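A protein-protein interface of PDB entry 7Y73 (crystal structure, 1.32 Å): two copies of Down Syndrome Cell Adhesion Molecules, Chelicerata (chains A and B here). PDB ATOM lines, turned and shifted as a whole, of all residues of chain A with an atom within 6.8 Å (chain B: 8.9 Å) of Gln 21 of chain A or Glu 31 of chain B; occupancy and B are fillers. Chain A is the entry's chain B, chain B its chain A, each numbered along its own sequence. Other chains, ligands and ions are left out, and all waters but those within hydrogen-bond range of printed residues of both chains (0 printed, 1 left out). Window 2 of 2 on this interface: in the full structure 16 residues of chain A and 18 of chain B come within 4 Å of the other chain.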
ATOM      1  N   THR A  16      19.525 -29.979   2.976  1.00  0.00           N
ATOM      2  CA  THR A  16      20.836 -29.394   3.221  1.00  0.00           C
ATOM      3  C   THR A  16      20.919 -27.950   2.738  1.00  0.00           C
ATOM      4  O   THR A  16      22.017 -27.450   2.472  1.00  0.00           O
ATOM      5  CB  THR A  16      21.915 -30.244   2.552  1.00  0.00           C
ATOM      6  OG1 THR A  16      21.570 -30.448   1.176  1.00  0.00           O
ATOM      7  CG2 THR A  16      22.039 -31.596   3.245  1.00  0.00           C
ATOM      8  N   LEU A  17      19.782 -27.277   2.608  1.00  0.00           N
ATOM      9  CA  LEU A  17      19.770 -25.862   2.271  1.00  0.00           C
ATOM     10  C   LEU A  17      20.071 -25.042   3.518  1.00  0.00           C
ATOM     11  O   LEU A  17      19.657 -25.397   4.626  1.00  0.00           O
ATOM     12  CB  LEU A  17      18.400 -25.471   1.721  1.00  0.00           C
ATOM     13  CG  LEU A  17      17.882 -26.327   0.564  1.00  0.00           C
ATOM     14  CD1 LEU A  17      16.416 -26.047   0.284  1.00  0.00           C
ATOM     15  CD2 LEU A  17      18.727 -26.075  -0.679  1.00  0.00           C
ATOM     16  N   HIS A  18      20.791 -23.937   3.334  1.00  0.00           N
ATOM     17  CA  HIS A  18      21.264 -23.127   4.444  1.00  0.00           C
ATOM     18  C   HIS A  18      20.780 -21.689   4.319  1.00  0.00           C
ATOM     19  O   HIS A  18      20.613 -21.161   3.216  1.00  0.00           O
ATOM     20  CB  HIS A  18      22.800 -23.147   4.514  1.00  0.00           C
ATOM     21  CG  HIS A  18      23.372 -24.512   4.730  1.00  0.00           C
ATOM     22  ND1 HIS A  18      23.404 -25.116   5.968  1.00  0.00           N
ATOM     23  CD2 HIS A  18      23.923 -25.397   3.866  1.00  0.00           C
ATOM     24  CE1 HIS A  18      23.955 -26.311   5.859  1.00  0.00           C
ATOM     25  NE2 HIS A  18      24.278 -26.507   4.593  1.00  0.00           N
ATOM     26  N   GLU A  19      20.552 -21.065   5.471  1.00  0.00           N
ATOM     27  CA  GLU A  19      20.097 -19.684   5.519  1.00  0.00           C
ATOM     28  C   GLU A  19      20.925 -18.816   4.582  1.00  0.00           C
ATOM     29  O   GLU A  19      22.155 -18.895   4.568  1.00  0.00           O
ATOM     30  CB  GLU A  19      20.244 -19.182   6.955  1.00  0.00           C
ATOM     31  CG  GLU A  19      19.419 -17.966   7.294  1.00  0.00           C
ATOM     32  CD  GLU A  19      19.611 -17.535   8.734  1.00  0.00           C
ATOM     33  OE1 GLU A  19      19.817 -18.416   9.596  1.00  0.00           O
ATOM     34  OE2 GLU A  19      19.562 -16.316   9.001  1.00  0.00           O
ATOM     35  N   GLY A  20      20.235 -18.001   3.782  1.00  0.00           N
ATOM     36  CA  GLY A  20      20.870 -17.079   2.867  1.00  0.00           C
ATOM     37  C   GLY A  20      21.030 -17.594   1.451  1.00  0.00           C
ATOM     38  O   GLY A  20      21.275 -16.793   0.537  1.00  0.00           O
ATOM     39  N   GLN A  21      20.894 -18.895   1.241  1.00  0.00           N
ATOM     40  CA  GLN A  21      21.044 -19.444  -0.093  1.00  0.00           C
ATOM     41  C   GLN A  21      19.774 -19.234  -0.907  1.00  0.00           C
ATOM     42  O   GLN A  21      18.682 -19.026  -0.371  1.00  0.00           O
ATOM     43  CB  GLN A  21      21.335 -20.941  -0.016  1.00  0.00           C
ATOM     44  CG  GLN A  21      22.685 -21.265   0.569  1.00  0.00           C
ATOM     45  CD  GLN A  21      22.997 -22.742   0.531  1.00  0.00           C
ATOM     46  OE1 GLN A  21      22.121 -23.576   0.748  1.00  0.00           O
ATOM     47  NE2 GLN A  21      24.253 -23.075   0.249  1.00  0.00           N
ATOM     48  N   THR A  22      19.933 -19.285  -2.227  1.00  0.00           N
ATOM     49  CA  THR A  22      18.797 -19.365  -3.129  1.00  0.00           C
ATOM     50  C   THR A  22      18.359 -20.819  -3.226  1.00  0.00           C
ATOM     51  O   THR A  22      19.193 -21.718  -3.373  1.00  0.00           O
ATOM     52  CB  THR A  22      19.201 -18.857  -4.511  1.00  0.00           C
ATOM     53  OG1 THR A  22      19.572 -17.477  -4.424  1.00  0.00           O
ATOM     54  CG2 THR A  22      18.054 -19.016  -5.501  1.00  0.00           C
ATOM     55  N   VAL A  23      17.056 -21.051  -3.144  1.00  0.00           N
ATOM     56  CA  VAL A  23      16.493 -22.389  -3.253  1.00  0.00           C
ATOM     57  C   VAL A  23      15.353 -22.349  -4.257  1.00  0.00           C
ATOM     58  O   VAL A  23      14.613 -21.361  -4.334  1.00  0.00           O
ATOM     59  CB  VAL A  23      16.018 -22.910  -1.881  1.00  0.00           C
ATOM     60  CG1 VAL A  23      17.090 -22.659  -0.823  1.00  0.00           C
ATOM     61  CG2 VAL A  23      14.714 -22.256  -1.483  1.00  0.00           C
ATOM     62  N   VAL A  66      13.038 -19.019  -4.128  1.00  0.00           N
ATOM     63  CA  VAL A  66      13.096 -18.307  -2.859  1.00  0.00           C
ATOM     64  C   VAL A  66      14.549 -17.909  -2.658  1.00  0.00           C
ATOM     65  O   VAL A  66      15.393 -18.753  -2.341  1.00  0.00           O
ATOM     66  CB  VAL A  66      12.604 -19.181  -1.696  1.00  0.00           C
ATOM     67  CG1 VAL A  66      12.900 -18.501  -0.370  1.00  0.00           C
ATOM     68  CG2 VAL A  66      11.120 -19.473  -1.846  1.00  0.00           C
ATOM     69  N   SER A  67      14.855 -16.636  -2.850  1.00  0.00           N
ATOM     70  CA  SER A  67      16.217 -16.158  -2.661  1.00  0.00           C
ATOM     71  C   SER A  67      16.434 -15.747  -1.208  1.00  0.00           C
ATOM     72  O   SER A  67      15.490 -15.412  -0.489  1.00  0.00           O
ATOM     73  CB  SER A  67      16.508 -14.984  -3.594  1.00  0.00           C
ATOM     74  OG  SER A  67      16.298 -15.371  -4.938  1.00  0.00           O
ATOM     75  N   SER A  68      17.689 -15.822  -0.778  1.00  0.00           N
ATOM     76  CA  SER A  68      18.080 -15.524   0.596  1.00  0.00           C
ATOM     77  C   SER A  68      17.138 -16.202   1.589  1.00  0.00           C
ATOM     78  O   SER A  68      16.479 -15.559   2.409  1.00  0.00           O
ATOM     79  CB  SER A  68      18.158 -14.014   0.826  1.00  0.00           C
ATOM     80  OG  SER A  68      18.534 -13.724   2.158  1.00  0.00           O
ATOM     81  N   VAL A  69      17.089 -17.533   1.503  1.00  0.00           N
ATOM     82  CA  VAL A  69      16.127 -18.288   2.297  1.00  0.00           C
ATOM     83  C   VAL A  69      16.343 -18.007   3.776  1.00  0.00           C
ATOM     84  O   VAL A  69      17.478 -17.891   4.253  1.00  0.00           O
ATOM     85  CB  VAL A  69      16.213 -19.792   1.978  1.00  0.00           C
ATOM     86  CG1 VAL A  69      17.564 -20.360   2.380  1.00  0.00           C
ATOM     87  CG2 VAL A  69      15.069 -20.543   2.664  1.00  0.00           C
ATOM     88  N   GLY A  70      15.243 -17.894   4.510  1.00  0.00           N
ATOM     89  CA  GLY A  70      15.324 -17.613   5.925  1.00  0.00           C
ATOM     90  C   GLY A  70      14.077 -18.063   6.651  1.00  0.00           C
ATOM     91  O   GLY A  70      13.232 -18.770   6.100  1.00  0.00           O
ATOM     92  N   ALA B   2      35.855 -18.795  -0.012  1.00  0.00           N
ATOM     93  CA  ALA B   2      36.081 -18.521  -1.428  1.00  0.00           C
ATOM     94  C   ALA B   2      34.875 -17.786  -2.004  1.00  0.00           C
ATOM     95  O   ALA B   2      34.066 -18.374  -2.722  1.00  0.00           O
ATOM     96  CB  ALA B   2      36.319 -19.813  -2.182  1.00  0.00           C
ATOM     97  N   SER B   3      34.761 -16.498  -1.690  1.00  0.00           N
ATOM     98  CA  SER B   3      33.584 -15.736  -2.088  1.00  0.00           C
ATOM     99  C   SER B   3      33.474 -15.665  -3.605  1.00  0.00           C
ATOM    100  O   SER B   3      34.469 -15.478  -4.313  1.00  0.00           O
ATOM    101  CB  SER B   3      33.657 -14.329  -1.496  1.00  0.00           C
ATOM    102  OG  SER B   3      33.929 -14.379  -0.104  1.00  0.00           O
ATOM    103  N   GLY B   4      32.247 -15.819  -4.102  1.00  0.00           N
ATOM    104  CA  GLY B   4      31.970 -15.844  -5.516  1.00  0.00           C
ATOM    105  C   GLY B   4      31.884 -17.234  -6.113  1.00  0.00           C
ATOM    106  O   GLY B   4      31.282 -17.399  -7.183  1.00  0.00           O
ATOM    107  N   ALA B   5      32.465 -18.229  -5.455  1.00  0.00           N
ATOM    108  CA  ALA B   5      32.452 -19.578  -5.987  1.00  0.00           C
ATOM    109  C   ALA B   5      31.020 -20.103  -6.065  1.00  0.00           C
ATOM    110  O   ALA B   5      30.182 -19.785  -5.214  1.00  0.00           O
ATOM    111  CB  ALA B   5      33.285 -20.502  -5.101  1.00  0.00           C
ATOM    112  N   PRO B   6      30.712 -20.920  -7.070  1.00  0.00           N
ATOM    113  CA  PRO B   6      29.352 -21.443  -7.207  1.00  0.00           C
ATOM    114  C   PRO B   6      29.133 -22.702  -6.385  1.00  0.00           C
ATOM    115  O   PRO B   6      30.034 -23.509  -6.165  1.00  0.00           O
ATOM    116  CB  PRO B   6      29.266 -21.761  -8.708  1.00  0.00           C
ATOM    117  CG  PRO B   6      30.666 -22.188  -9.065  1.00  0.00           C
ATOM    118  CD  PRO B   6      31.601 -21.385  -8.155  1.00  0.00           C
ATOM    119  N   LYS B   7      27.905 -22.847  -5.913  1.00  0.00           N
ATOM    120  CA  LYS B   7      27.456 -24.065  -5.260  1.00  0.00           C
ATOM    121  C   LYS B   7      26.099 -24.426  -5.832  1.00  0.00           C
ATOM    122  O   LYS B   7      25.295 -23.548  -6.180  1.00  0.00           O
ATOM    123  CB  LYS B   7      27.379 -23.908  -3.741  1.00  0.00           C
ATOM    124  CG  LYS B   7      28.747 -23.697  -3.089  1.00  0.00           C
ATOM    125  CD  LYS B   7      28.678 -23.862  -1.580  1.00  0.00           C
ATOM    126  CE  LYS B   7      29.849 -23.178  -0.874  1.00  0.00           C
ATOM    127  NZ  LYS B   7      30.639 -22.242  -1.730  1.00  0.00           N
ATOM    128  N   LEU B   8      25.857 -25.725  -5.955  1.00  0.00           N
ATOM    129  CA  LEU B   8      24.654 -26.238  -6.589  1.00  0.00           C
ATOM    130  C   LEU B   8      23.649 -26.712  -5.552  1.00  0.00           C
ATOM    131  O   LEU B   8      24.017 -27.261  -4.509  1.00  0.00           O
ATOM    132  CB  LEU B   8      24.989 -27.406  -7.517  1.00  0.00           C
ATOM    133  CG  LEU B   8      25.722 -27.032  -8.804  1.00  0.00           C
ATOM    134  CD1 LEU B   8      26.142 -28.291  -9.556  1.00  0.00           C
ATOM    135  CD2 LEU B   8      24.861 -26.140  -9.671  1.00  0.00           C
ATOM    136  N   GLN B   9      22.377 -26.504  -5.847  1.00  0.00           N
ATOM    137  CA  GLN B   9      21.323 -27.145  -5.083  1.00  0.00           C
ATOM    138  C   GLN B   9      21.379 -28.639  -5.363  1.00  0.00           C
ATOM    139  O   GLN B   9      21.328 -29.042  -6.537  1.00  0.00           O
ATOM    140  CB  GLN B   9      19.975 -26.592  -5.513  1.00  0.00           C
ATOM    141  CG  GLN B   9      18.830 -27.162  -4.706  1.00  0.00           C
ATOM    142  CD  GLN B   9      17.526 -26.445  -4.953  1.00  0.00           C
ATOM    143  OE1 GLN B   9      17.473 -25.216  -4.950  1.00  0.00           O
ATOM    144  NE2 GLN B   9      16.457 -27.212  -5.157  1.00  0.00           N
ATOM    145  N   PRO B  10      21.503 -29.492  -4.347  1.00  0.00           N
ATOM    146  CA  PRO B  10      21.492 -30.936  -4.613  1.00  0.00           C
ATOM    147  C   PRO B  10      20.204 -31.344  -5.305  1.00  0.00           C
ATOM    148  O   PRO B  10      19.120 -30.852  -4.980  1.00  0.00           O
ATOM    149  CB  PRO B  10      21.603 -31.566  -3.219  1.00  0.00           C
ATOM    150  CG  PRO B  10      22.140 -30.481  -2.333  1.00  0.00           C
ATOM    151  CD  PRO B  10      21.608 -29.190  -2.908  1.00  0.00           C
ATOM    152  N   THR B  28      20.898 -25.931 -10.657  1.00  0.00           N
ATOM    153  CA  THR B  28      20.663 -24.540 -10.333  1.00  0.00           C
ATOM    154  C   THR B  28      21.497 -24.158  -9.119  1.00  0.00           C
ATOM    155  O   THR B  28      21.653 -24.969  -8.190  1.00  0.00           O
ATOM    156  CB  THR B  28      19.159 -24.325 -10.077  1.00  0.00           C
ATOM    157  OG1 THR B  28      18.863 -22.925 -10.034  1.00  0.00           O
ATOM    158  CG2 THR B  28      18.695 -25.011  -8.800  1.00  0.00           C
ATOM    159  N   PRO B  29      22.074 -22.954  -9.116  1.00  0.00           N
ATOM    160  CA  PRO B  29      23.021 -22.596  -8.056  1.00  0.00           C
ATOM    161  C   PRO B  29      22.358 -21.972  -6.839  1.00  0.00           C
ATOM    162  O   PRO B  29      21.456 -21.138  -6.937  1.00  0.00           O
ATOM    163  CB  PRO B  29      23.926 -21.572  -8.752  1.00  0.00           C
ATOM    164  CG  PRO B  29      22.973 -20.854  -9.695  1.00  0.00           C
ATOM    165  CD  PRO B  29      22.021 -21.933 -10.187  1.00  0.00           C
ATOM    166  N   THR B  30      22.829 -22.393  -5.664  1.00  0.00           N
ATOM    167  CA  THR B  30      22.391 -21.791  -4.412  1.00  0.00           C
ATOM    168  C   THR B  30      23.145 -20.506  -4.108  1.00  0.00           C
ATOM    169  O   THR B  30      22.639 -19.664  -3.356  1.00  0.00           O
ATOM    170  CB  THR B  30      22.624 -22.766  -3.261  1.00  0.00           C
ATOM    171  OG1 THR B  30      23.986 -23.213  -3.304  1.00  0.00           O
ATOM    172  CG2 THR B  30      21.687 -23.954  -3.374  1.00  0.00           C
ATOM    173  N   GLU B  31      24.345 -20.355  -4.661  1.00  0.00           N
ATOM    174  CA  GLU B  31      25.139 -19.151  -4.465  1.00  0.00           C
ATOM    175  C   GLU B  31      26.170 -19.076  -5.579  1.00  0.00           C
ATOM    176  O   GLU B  31      26.403 -20.051  -6.303  1.00  0.00           O
ATOM    177  CB  GLU B  31      25.820 -19.145  -3.093  1.00  0.00           C
ATOM    178  CG  GLU B  31      26.548 -20.423  -2.739  1.00  0.00           C
ATOM    179  CD  GLU B  31      27.013 -20.446  -1.290  1.00  0.00           C
ATOM    180  OE1 GLU B  31      28.173 -20.068  -1.035  1.00  0.00           O
ATOM    181  OE2 GLU B  31      26.223 -20.844  -0.409  1.00  0.00           O
ATOM    182  N   GLY B  32      26.761 -17.897  -5.721  1.00  0.00           N
ATOM    183  CA  GLY B  32      27.824 -17.692  -6.683  1.00  0.00           C
ATOM    184  C   GLY B  32      27.699 -16.410  -7.466  1.00  0.00           C
ATOM    185  O   GLY B  32      26.680 -15.702  -7.362  1.00  0.00           O
ATOM    186  N   GLU B  33      28.732 -16.101  -8.247  1.00  0.00           N
ATOM    187  CA  GLU B  33      28.789 -14.931  -9.101  1.00  0.00           C
ATOM    188  C   GLU B  33      28.814 -15.376 -10.546  1.00  0.00           C
ATOM    189  O   GLU B  33      29.511 -16.339 -10.891  1.00  0.00           O
ATOM    190  CB  GLU B  33      30.102 -14.160  -8.828  1.00  0.00           C
ATOM    191  CG  GLU B  33      30.081 -13.299  -7.617  1.00  0.00           C
ATOM    192  CD  GLU B  33      28.946 -12.367  -7.724  1.00  0.00           C
ATOM    193  OE1 GLU B  33      28.389 -12.033  -8.730  1.00  0.00           O
ATOM    194  OE2 GLU B  33      28.473 -11.909  -6.772  1.00  0.00           O
ATOM    195  N   ARG B  34      28.100 -14.653 -11.404  1.00  0.00           N
ATOM    196  CA  ARG B  34      28.220 -14.877 -12.833  1.00  0.00           C
ATOM    197  C   ARG B  34      29.491 -14.211 -13.354  1.00  0.00           C
ATOM    198  O   ARG B  34      30.030 -13.304 -12.718  1.00  0.00           O
ATOM    199  CB  ARG B  34      26.981 -14.340 -13.542  1.00  0.00           C
ATOM    200  CG  ARG B  34      25.741 -15.158 -13.187  1.00  0.00           C
ATOM    201  CD  ARG B  34      24.453 -14.441 -13.526  1.00  0.00           C
ATOM    202  NE  ARG B  34      24.347 -14.233 -14.965  1.00  0.00           N
ATOM    203  CZ  ARG B  34      23.262 -13.786 -15.583  1.00  0.00           C
ATOM    204  NH1 ARG B  34      22.175 -13.498 -14.886  1.00  0.00           N
ATOM    205  NH2 ARG B  34      23.266 -13.631 -16.898  1.00  0.00           N
ATOM    206  N   LEU B  36      28.643 -17.966 -15.003  1.00  0.00           N
ATOM    207  CA  LEU B  36      28.706 -19.378 -14.661  1.00  0.00           C
ATOM    208  C   LEU B  36      28.652 -20.203 -15.936  1.00  0.00           C
ATOM    209  O   LEU B  36      27.978 -19.843 -16.899  1.00  0.00           O
ATOM    210  CB  LEU B  36      27.508 -19.792 -13.809  1.00  0.00           C
ATOM    211  CG  LEU B  36      27.333 -19.118 -12.459  1.00  0.00           C
ATOM    212  CD1 LEU B  36      26.114 -19.708 -11.755  1.00  0.00           C
ATOM    213  CD2 LEU B  36      28.566 -19.280 -11.606  1.00  0.00           C
ATOM    214  N   PHE B  38      27.898 -24.257 -17.189  1.00  0.00           N
ATOM    215  CA  PHE B  38      27.299 -25.517 -16.794  1.00  0.00           C
ATOM    216  C   PHE B  38      27.635 -26.571 -17.837  1.00  0.00           C
ATOM    217  O   PHE B  38      27.732 -26.269 -19.030  1.00  0.00           O
ATOM    218  CB  PHE B  38      25.763 -25.399 -16.712  1.00  0.00           C
ATOM    219  CG  PHE B  38      25.285 -24.494 -15.616  1.00  0.00           C
ATOM    220  CD1 PHE B  38      24.937 -25.010 -14.381  1.00  0.00           C
ATOM    221  CD2 PHE B  38      25.187 -23.126 -15.818  1.00  0.00           C
ATOM    222  CE1 PHE B  38      24.514 -24.182 -13.369  1.00  0.00           C
ATOM    223  CE2 PHE B  38      24.758 -22.296 -14.804  1.00  0.00           C
ATOM    224  CZ  PHE B  38      24.415 -22.827 -13.580  1.00  0.00           C
ATOM    225  N   ASP B  60      21.272 -18.402 -15.699  1.00  0.00           N
ATOM    226  CA  ASP B  60      22.220 -18.851 -14.680  1.00  0.00           C
ATOM    227  C   ASP B  60      21.838 -20.205 -14.077  1.00  0.00           C
ATOM    228  O   ASP B  60      22.149 -20.471 -12.911  1.00  0.00           O
ATOM    229  CB  ASP B  60      22.398 -17.783 -13.582  1.00  0.00           C
ATOM    230  CG  ASP B  60      21.096 -17.425 -12.873  1.00  0.00           C
ATOM    231  OD1 ASP B  60      21.132 -16.553 -11.976  1.00  0.00           O
ATOM    232  OD2 ASP B  60      20.038 -17.990 -13.220  1.00  0.00           O
ATOM    233  N   VAL B  81      29.155 -27.080 -12.437  1.00  0.00           N
ATOM    234  CA  VAL B  81      29.138 -25.637 -12.634  1.00  0.00           C
ATOM    235  C   VAL B  81      30.523 -25.109 -12.296  1.00  0.00           C
ATOM    236  O   VAL B  81      31.172 -25.596 -11.365  1.00  0.00           O
ATOM    237  CB  VAL B  81      28.042 -24.953 -11.787  1.00  0.00           C
ATOM    238  CG1 VAL B  81      28.308 -25.126 -10.304  1.00  0.00           C
ATOM    239  CG2 VAL B  81      27.921 -23.473 -12.145  1.00  0.00           C
ATOM    240  N   ASN B  83      33.178 -21.378 -12.387  1.00  0.00           N
ATOM    241  CA  ASN B  83      33.483 -19.982 -12.696  1.00  0.00           C
ATOM    242  C   ASN B  83      34.925 -19.719 -12.271  1.00  0.00           C
ATOM    243  O   ASN B  83      35.647 -20.636 -11.872  1.00  0.00           O
ATOM    244  CB  ASN B  83      32.443 -19.016 -12.102  1.00  0.00           C
ATOM    245  CG  ASN B  83      32.517 -18.919 -10.597  1.00  0.00           C
ATOM    246  OD1 ASN B  83      33.443 -19.430  -9.968  1.00  0.00           O
ATOM    247  ND2 ASN B  83      31.534 -18.249 -10.009  1.00  0.00           N
ATOM    248  N   SER B  87      34.226 -24.467  -8.453  1.00  0.00           N
ATOM    249  CA  SER B  87      33.327 -25.358  -9.164  1.00  0.00           C
ATOM    250  C   SER B  87      32.537 -26.163  -8.143  1.00  0.00           C
ATOM    251  O   SER B  87      32.872 -26.202  -6.960  1.00  0.00           O
ATOM    252  CB  SER B  87      34.113 -26.291 -10.091  1.00  0.00           C
ATOM    253  OG  SER B  87      34.922 -27.184  -9.346  1.00  0.00           O
ATOM    254  N   ASP B  88      31.464 -26.787  -8.614  1.00  0.00           N
ATOM    255  CA  ASP B  88      30.672 -27.692  -7.800  1.00  0.00           C
ATOM    256  C   ASP B  88      29.998 -28.665  -8.752  1.00  0.00           C
ATOM    257  O   ASP B  88      29.928 -28.423  -9.962  1.00  0.00           O
ATOM    258  CB  ASP B  88      29.653 -26.944  -6.938  1.00  0.00           C
ATOM    259  CG  ASP B  88      29.121 -27.789  -5.794  1.00  0.00           C
ATOM    260  OD1 ASP B  88      29.775 -28.784  -5.401  1.00  0.00           O
ATOM    261  OD2 ASP B  88      28.042 -27.443  -5.276  1.00  0.00           O
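No position is printed for both chains.
Of the printed residues of chain B, Gln 21 of chain A touches Thr 30 and Glu 31. Glu 31 of chain B touches one residue of chain A. Of the printed residues of chain B, Thr 16 of chain A touches Pro 10. Of the printed residues of chain A, Pro 10 of chain B touches Thr 16. The nearest residue of chain B that does not touch Gln 21 of chain A is Lys 7 of chain B (4.9 Å). The nearest printed residue of chain A that does not touch Pro 10 of chain B is Leu 17 of chain A (4.8 Å).
The backbone NH of Val 66 of chain A is in hydrogen-bond range of the backbone carbonyl oxygen of Val 23 of chain A (2.8 Å). OE1 of Glu 31 of chain B is in salt-bridge range of NZ of Lys 7 of chain B (3.4 Å). N of Ser 68 of chain A sits at hydrogen-bond distance from O of Gln 21 of chain A. The backbone carbonyl oxygen (O) of Lys 7 of chain B sits at hydrogen-bond distance from the backbone NH (N) of Thr 30 of chain B, at 2.8 Å. O of Thr 16 of chain A lies close to NE2 of His 18 of chain A, at 3.2 Å. The backbone carbonyl oxygen (O) of Gln 21 of chain A is in hydrogen-bond range of the backbone NH (N) of Val 69 of chain A, at 2.9 Å.
Of the 23 printed residues of chain B, 4 touch a printed residue of chain A. Printed residues of chain A that touch a printed residue of chain B: Thr 16, Gln 21, Thr 22 and Val 23. Among the printed residues, 5 pairs touch across the chains. Among the printed residues, no Asp or Glu carboxylate lies within 4 Å of a Lys or Arg side-chain nitrogen of the other chain.
Pro 10 of chain B touches Thr 16 of chain A (CG to OG1, 3.6 Å). Thr 30 of chain B touches Gln 21 of chain A (OG1 to NE2, 3.6 Å). Gln 9 of chain B touches Val 23 of chain A.
O of Thr 30 of chain B sits at hydrogen-bond distance from N of Thr 22 of chain A (3.0 Å). The side-chain carboxylate (OE2) of Glu 31 of chain B sits at hydrogen-bond distance from the side-chain amide nitrogen (NE2) of Gln 21 of chain A (3.0 Å).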
